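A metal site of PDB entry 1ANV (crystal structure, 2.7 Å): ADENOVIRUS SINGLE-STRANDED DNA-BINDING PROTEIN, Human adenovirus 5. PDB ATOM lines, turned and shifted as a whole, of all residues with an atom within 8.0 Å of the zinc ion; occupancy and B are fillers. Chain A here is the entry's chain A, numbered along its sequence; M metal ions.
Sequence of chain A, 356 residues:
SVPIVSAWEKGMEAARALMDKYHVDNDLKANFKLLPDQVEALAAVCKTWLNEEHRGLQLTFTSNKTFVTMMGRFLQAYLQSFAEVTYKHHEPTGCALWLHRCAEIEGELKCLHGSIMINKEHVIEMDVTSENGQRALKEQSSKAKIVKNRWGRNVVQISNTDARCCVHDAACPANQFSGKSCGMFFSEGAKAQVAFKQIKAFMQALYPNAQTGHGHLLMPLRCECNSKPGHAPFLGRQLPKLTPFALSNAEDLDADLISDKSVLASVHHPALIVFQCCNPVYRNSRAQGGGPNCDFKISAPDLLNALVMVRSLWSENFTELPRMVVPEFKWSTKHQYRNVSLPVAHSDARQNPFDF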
ATOM      1  N   ARG A 222     -13.703 -16.892  -3.025  1.00  0.00           N
ATOM      2  CA  ARG A 222     -13.542 -18.099  -3.806  1.00  0.00           C
ATOM      3  C   ARG A 222     -12.319 -18.887  -3.459  1.00  0.00           C
ATOM      4  O   ARG A 222     -11.302 -18.339  -3.037  1.00  0.00           O
ATOM      5  CB  ARG A 222     -13.597 -17.862  -5.322  1.00  0.00           C
ATOM      6  CG  ARG A 222     -12.711 -16.733  -5.804  1.00  0.00           C
ATOM      7  CD  ARG A 222     -13.013 -16.322  -7.233  1.00  0.00           C
ATOM      8  NE  ARG A 222     -11.832 -15.727  -7.879  1.00  0.00           N
ATOM      9  CZ  ARG A 222     -11.780 -14.495  -8.365  1.00  0.00           C
ATOM     10  NH1 ARG A 222     -12.826 -13.674  -8.309  1.00  0.00           N
ATOM     11  NH2 ARG A 222     -10.655 -14.071  -8.916  1.00  0.00           N
ATOM     12  N   CYS A 223     -12.458 -20.179  -3.628  1.00  0.00           N
ATOM     13  CA  CYS A 223     -11.379 -21.077  -3.362  1.00  0.00           C
ATOM     14  C   CYS A 223     -10.979 -21.722  -4.662  1.00  0.00           C
ATOM     15  O   CYS A 223     -11.278 -21.247  -5.756  1.00  0.00           O
ATOM     16  CB  CYS A 223     -11.746 -22.174  -2.356  1.00  0.00           C
ATOM     17  SG  CYS A 223     -13.043 -23.247  -2.949  1.00  0.00           S
ATOM     18  N   GLU A 224     -10.299 -22.831  -4.518  1.00  0.00           N
ATOM     19  CA  GLU A 224      -9.886 -23.538  -5.698  1.00  0.00           C
ATOM     20  C   GLU A 224     -11.114 -23.948  -6.489  1.00  0.00           C
ATOM     21  O   GLU A 224     -11.143 -23.889  -7.701  1.00  0.00           O
ATOM     22  CB  GLU A 224      -9.015 -24.751  -5.295  1.00  0.00           C
ATOM     23  CG  GLU A 224      -8.332 -25.484  -6.457  1.00  0.00           C
ATOM     24  CD  GLU A 224      -7.885 -26.845  -6.029  1.00  0.00           C
ATOM     25  OE1 GLU A 224      -6.828 -26.818  -5.252  1.00  0.00           O
ATOM     26  OE2 GLU A 224      -8.457 -27.871  -6.364  1.00  0.00           O
ATOM     27  N   CYS A 225     -12.171 -24.342  -5.794  1.00  0.00           N
ATOM     28  CA  CYS A 225     -13.379 -24.777  -6.445  1.00  0.00           C
ATOM     29  C   CYS A 225     -14.083 -23.786  -7.347  1.00  0.00           C
ATOM     30  O   CYS A 225     -14.475 -24.125  -8.460  1.00  0.00           O
ATOM     31  CB  CYS A 225     -14.306 -25.444  -5.464  1.00  0.00           C
ATOM     32  SG  CYS A 225     -13.335 -26.678  -4.582  1.00  0.00           S
ATOM     33  N   ASN A 226     -14.270 -22.586  -6.875  1.00  0.00           N
ATOM     34  CA  ASN A 226     -14.946 -21.593  -7.679  1.00  0.00           C
ATOM     35  C   ASN A 226     -13.953 -20.579  -8.170  1.00  0.00           C
ATOM     36  O   ASN A 226     -14.248 -19.412  -8.349  1.00  0.00           O
ATOM     37  CB  ASN A 226     -16.086 -20.925  -6.895  1.00  0.00           C
ATOM     38  CG  ASN A 226     -15.609 -20.475  -5.540  1.00  0.00           C
ATOM     39  OD1 ASN A 226     -14.479 -20.824  -5.141  1.00  0.00           O
ATOM     40  ND2 ASN A 226     -16.436 -19.692  -4.871  1.00  0.00           N
ATOM     41  N   SER A 227     -12.737 -21.055  -8.366  1.00  0.00           N
ATOM     42  CA  SER A 227     -11.678 -20.186  -8.824  1.00  0.00           C
ATOM     43  C   SER A 227     -12.007 -19.472 -10.135  1.00  0.00           C
ATOM     44  O   SER A 227     -11.658 -18.321 -10.348  1.00  0.00           O
ATOM     45  CB  SER A 227     -10.415 -20.987  -9.054  1.00  0.00           C
ATOM     46  OG  SER A 227     -10.664 -21.875 -10.127  1.00  0.00           O
ATOM     47  N   PHE A 234     -21.676 -26.063  -8.407  1.00  0.00           N
ATOM     48  CA  PHE A 234     -21.614 -27.118  -7.416  1.00  0.00           C
ATOM     49  C   PHE A 234     -22.499 -26.812  -6.226  1.00  0.00           C
ATOM     50  O   PHE A 234     -22.658 -25.648  -5.843  1.00  0.00           O
ATOM     51  CB  PHE A 234     -20.168 -27.487  -7.008  1.00  0.00           C
ATOM     52  CG  PHE A 234     -19.407 -26.341  -6.391  1.00  0.00           C
ATOM     53  CD1 PHE A 234     -19.527 -26.049  -5.040  1.00  0.00           C
ATOM     54  CD2 PHE A 234     -18.568 -25.535  -7.174  1.00  0.00           C
ATOM     55  CE1 PHE A 234     -18.824 -25.004  -4.446  1.00  0.00           C
ATOM     56  CE2 PHE A 234     -17.873 -24.476  -6.611  1.00  0.00           C
ATOM     57  CZ  PHE A 234     -17.993 -24.210  -5.239  1.00  0.00           C
ATOM     58  N   ARG A 237     -22.104 -24.934   0.104  1.00  0.00           N
ATOM     59  CA  ARG A 237     -21.676 -23.578   0.385  1.00  0.00           C
ATOM     60  C   ARG A 237     -20.996 -22.977  -0.851  1.00  0.00           C
ATOM     61  O   ARG A 237     -20.126 -23.563  -1.484  1.00  0.00           O
ATOM     62  CB  ARG A 237     -20.821 -23.488   1.644  1.00  0.00           C
ATOM     63  CG  ARG A 237     -20.164 -22.119   1.802  1.00  0.00           C
ATOM     64  CD  ARG A 237     -19.424 -21.940   3.114  1.00  0.00           C
ATOM     65  NE  ARG A 237     -20.206 -22.406   4.263  1.00  0.00           N
ATOM     66  CZ  ARG A 237     -20.138 -23.637   4.742  1.00  0.00           C
ATOM     67  NH1 ARG A 237     -19.358 -24.556   4.213  1.00  0.00           N
ATOM     68  NH2 ARG A 237     -20.886 -23.960   5.789  1.00  0.00           N
ATOM     69  N   LEU A 239     -19.215 -20.195  -0.852  1.00  0.00           N
ATOM     70  CA  LEU A 239     -18.113 -19.340  -0.414  1.00  0.00           C
ATOM     71  C   LEU A 239     -17.213 -20.141   0.486  1.00  0.00           C
ATOM     72  O   LEU A 239     -17.612 -21.168   1.049  1.00  0.00           O
ATOM     73  CB  LEU A 239     -18.610 -18.165   0.451  1.00  0.00           C
ATOM     74  CG  LEU A 239     -18.984 -16.890  -0.290  1.00  0.00           C
ATOM     75  CD1 LEU A 239     -19.075 -15.720   0.697  1.00  0.00           C
ATOM     76  CD2 LEU A 239     -17.947 -16.558  -1.360  1.00  0.00           C
ATOM     77  N   PRO A 240     -16.005 -19.679   0.654  1.00  0.00           N
ATOM     78  CA  PRO A 240     -15.124 -20.414   1.510  1.00  0.00           C
ATOM     79  C   PRO A 240     -15.664 -20.389   2.922  1.00  0.00           C
ATOM     80  O   PRO A 240     -16.246 -19.389   3.348  1.00  0.00           O
ATOM     81  CB  PRO A 240     -13.741 -19.766   1.380  1.00  0.00           C
ATOM     82  CG  PRO A 240     -13.810 -18.874   0.148  1.00  0.00           C
ATOM     83  CD  PRO A 240     -15.291 -18.669  -0.161  1.00  0.00           C
ATOM     84  N   GLN A 276     -11.462 -22.053   4.763  1.00  0.00           N
ATOM     85  CA  GLN A 276     -11.099 -23.256   4.046  1.00  0.00           C
ATOM     86  C   GLN A 276     -11.858 -23.333   2.733  1.00  0.00           C
ATOM     87  O   GLN A 276     -12.252 -22.323   2.192  1.00  0.00           O
ATOM     88  CB  GLN A 276     -11.379 -24.513   4.851  1.00  0.00           C
ATOM     89  CG  GLN A 276     -10.550 -24.547   6.141  1.00  0.00           C
ATOM     90  CD  GLN A 276     -11.344 -25.106   7.290  1.00  0.00           C
ATOM     91  OE1 GLN A 276     -12.481 -24.672   7.550  1.00  0.00           O
ATOM     92  NE2 GLN A 276     -10.748 -26.090   7.963  1.00  0.00           N
ATOM     93  N   CYS A 277     -12.055 -24.549   2.223  1.00  0.00           N
ATOM     94  CA  CYS A 277     -12.777 -24.720   0.982  1.00  0.00           C
ATOM     95  C   CYS A 277     -14.213 -24.300   1.174  1.00  0.00           C
ATOM     96  O   CYS A 277     -14.641 -24.073   2.295  1.00  0.00           O
ATOM     97  CB  CYS A 277     -12.770 -26.207   0.555  1.00  0.00           C
ATOM     98  SG  CYS A 277     -13.446 -26.492  -1.109  1.00  0.00           S
ATOM     99  N   CYS A 278     -14.954 -24.216   0.072  1.00  0.00           N
ATOM    100  CA  CYS A 278     -16.355 -23.852   0.152  1.00  0.00           C
ATOM    101  C   CYS A 278     -17.058 -24.904   0.977  1.00  0.00           C
ATOM    102  O   CYS A 278     -17.923 -24.630   1.815  1.00  0.00           O
ATOM    103  CB  CYS A 278     -16.988 -23.747  -1.238  1.00  0.00           C
ATOM    104  SG  CYS A 278     -16.543 -22.207  -2.047  1.00  0.00           S
ATOM    105  N   ASN A 279     -16.622 -26.125   0.727  1.00  0.00           N
ATOM    106  CA  ASN A 279     -17.131 -27.271   1.404  1.00  0.00           C
ATOM    107  C   ASN A 279     -16.004 -28.239   1.691  1.00  0.00           C
ATOM    108  O   ASN A 279     -15.533 -28.933   0.793  1.00  0.00           O
ATOM    109  CB  ASN A 279     -18.211 -27.952   0.555  1.00  0.00           C
ATOM    110  CG  ASN A 279     -19.220 -26.964  -0.016  1.00  0.00           C
ATOM    111  OD1 ASN A 279     -20.069 -26.399   0.700  1.00  0.00           O
ATOM    112  ND2 ASN A 279     -19.144 -26.766  -1.318  1.00  0.00           N
ATOM    113  N   PRO A 280     -15.570 -28.274   2.945  1.00  0.00           N
ATOM    114  CA  PRO A 280     -14.497 -29.171   3.343  1.00  0.00           C
ATOM    115  C   PRO A 280     -15.070 -30.466   3.913  1.00  0.00           C
ATOM    116  O   PRO A 280     -14.471 -31.547   3.817  1.00  0.00           O
ATOM    117  CB  PRO A 280     -13.696 -28.414   4.420  1.00  0.00           C
ATOM    118  CG  PRO A 280     -14.569 -27.248   4.877  1.00  0.00           C
ATOM    119  CD  PRO A 280     -15.729 -27.154   3.895  1.00  0.00           C
ATOM    120  N   PRO A 292     -17.058 -31.260  -5.472  1.00  0.00           N
ATOM    121  CA  PRO A 292     -15.671 -30.848  -5.428  1.00  0.00           C
ATOM    122  C   PRO A 292     -15.248 -30.445  -4.027  1.00  0.00           C
ATOM    123  O   PRO A 292     -16.084 -30.079  -3.183  1.00  0.00           O
ATOM    124  CB  PRO A 292     -15.526 -29.673  -6.390  1.00  0.00           C
ATOM    125  CG  PRO A 292     -16.941 -29.237  -6.770  1.00  0.00           C
ATOM    126  CD  PRO A 292     -17.899 -30.223  -6.133  1.00  0.00           C
ATOM    127  N   ASN A 293     -13.947 -30.514  -3.797  1.00  0.00           N
ATOM    128  CA  ASN A 293     -13.306 -30.167  -2.540  1.00  0.00           C
ATOM    129  C   ASN A 293     -11.851 -29.812  -2.788  1.00  0.00           C
ATOM    130  O   ASN A 293     -11.142 -30.522  -3.491  1.00  0.00           O
ATOM    131  CB  ASN A 293     -13.372 -31.288  -1.484  1.00  0.00           C
ATOM    132  CG  ASN A 293     -12.286 -31.121  -0.417  1.00  0.00           C
ATOM    133  OD1 ASN A 293     -11.274 -31.836  -0.403  1.00  0.00           O
ATOM    134  ND2 ASN A 293     -12.487 -30.148   0.479  1.00  0.00           N
ATOM    135  N   CYS A 294     -11.392 -28.727  -2.187  1.00  0.00           N
ATOM    136  CA  CYS A 294     -10.005 -28.376  -2.367  1.00  0.00           C
ATOM    137  C   CYS A 294      -9.329 -28.270  -1.024  1.00  0.00           C
ATOM    138  O   CYS A 294     -10.014 -28.336  -0.004  1.00  0.00           O
ATOM    139  CB  CYS A 294      -9.766 -27.143  -3.243  1.00  0.00           C
ATOM    140  SG  CYS A 294     -10.382 -25.606  -2.515  1.00  0.00           S
ATOM    141  N   ASP A 295      -8.003 -28.125  -1.051  1.00  0.00           N
ATOM    142  CA  ASP A 295      -7.229 -28.014   0.175  1.00  0.00           C
ATOM    143  C   ASP A 295      -6.859 -26.568   0.525  1.00  0.00           C
ATOM    144  O   ASP A 295      -5.800 -26.287   1.122  1.00  0.00           O
ATOM    145  CB  ASP A 295      -6.054 -29.023   0.201  1.00  0.00           C
ATOM    146  CG  ASP A 295      -6.245 -30.136   1.191  1.00  0.00           C
ATOM    147  OD1 ASP A 295      -6.795 -31.196   0.932  1.00  0.00           O
ATOM    148  OD2 ASP A 295      -5.769 -29.858   2.378  1.00  0.00           O
ATOM    149  N   PHE A 296      -7.764 -25.654   0.173  1.00  0.00           N
ATOM    150  CA  PHE A 296      -7.616 -24.232   0.450  1.00  0.00           C
ATOM    151  C   PHE A 296      -7.681 -23.941   1.942  1.00  0.00           C
ATOM    152  O   PHE A 296      -8.636 -24.318   2.630  1.00  0.00           O
ATOM    153  CB  PHE A 296      -8.718 -23.450  -0.260  1.00  0.00           C
ATOM    154  CG  PHE A 296      -8.608 -21.947  -0.229  1.00  0.00           C
ATOM    155  CD1 PHE A 296      -9.197 -21.215   0.795  1.00  0.00           C
ATOM    156  CD2 PHE A 296      -7.988 -21.257  -1.272  1.00  0.00           C
ATOM    157  CE1 PHE A 296      -9.151 -19.829   0.784  1.00  0.00           C
ATOM    158  CE2 PHE A 296      -7.925 -19.857  -1.295  1.00  0.00           C
ATOM    159  CZ  PHE A 296      -8.512 -19.142  -0.252  1.00  0.00           C
HETATM  160 ZN    ZN M   1     -12.650 -25.511  -2.852  1.00  0.00          ZN
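The zinc ion is bound by SG of Cys 277 (2.2 Å), SG of Cys 225 (2.2 Å), SG of Cys 294 (2.3 Å) and SG of Cys 223 (2.3 Å).
Glu 224 touches the zinc ion (N to ZN, 3.9 Å). Cys 278 touches the zinc ion. The nearest printed residue that does not touch the zinc ion is Asn 293 (4.4 Å).
The backbone NH of Cys 277 sits at hydrogen-bond distance from the backbone carbonyl oxygen of Phe 296. SG of Cys 277 lies close to N of Asn 279, 3.7 Å away. SG of Cys 294 lies close to N of Glu 224, at 3.4 Å. The backbone NH (N) of Phe 296 sits close to the side-chain sulfur (SG) of Cys 294 (3.8 Å). The side-chain sulfur of Cys 223 sits close to the backbone NH of Cys 278. The side-chain amide oxygen (OD1) of Asn 226 lies within hydrogen-bond range of the backbone NH (N) of Cys 223. The side-chain hydroxyl (OG) of Ser 227 lies within hydrogen-bond range of the backbone carbonyl oxygen (O) of Glu 224 (3.2 Å). The side-chain sulfur (SG) of Cys 278 lies close to the backbone carbonyl oxygen (O) of Leu 239, at 3.4 Å.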
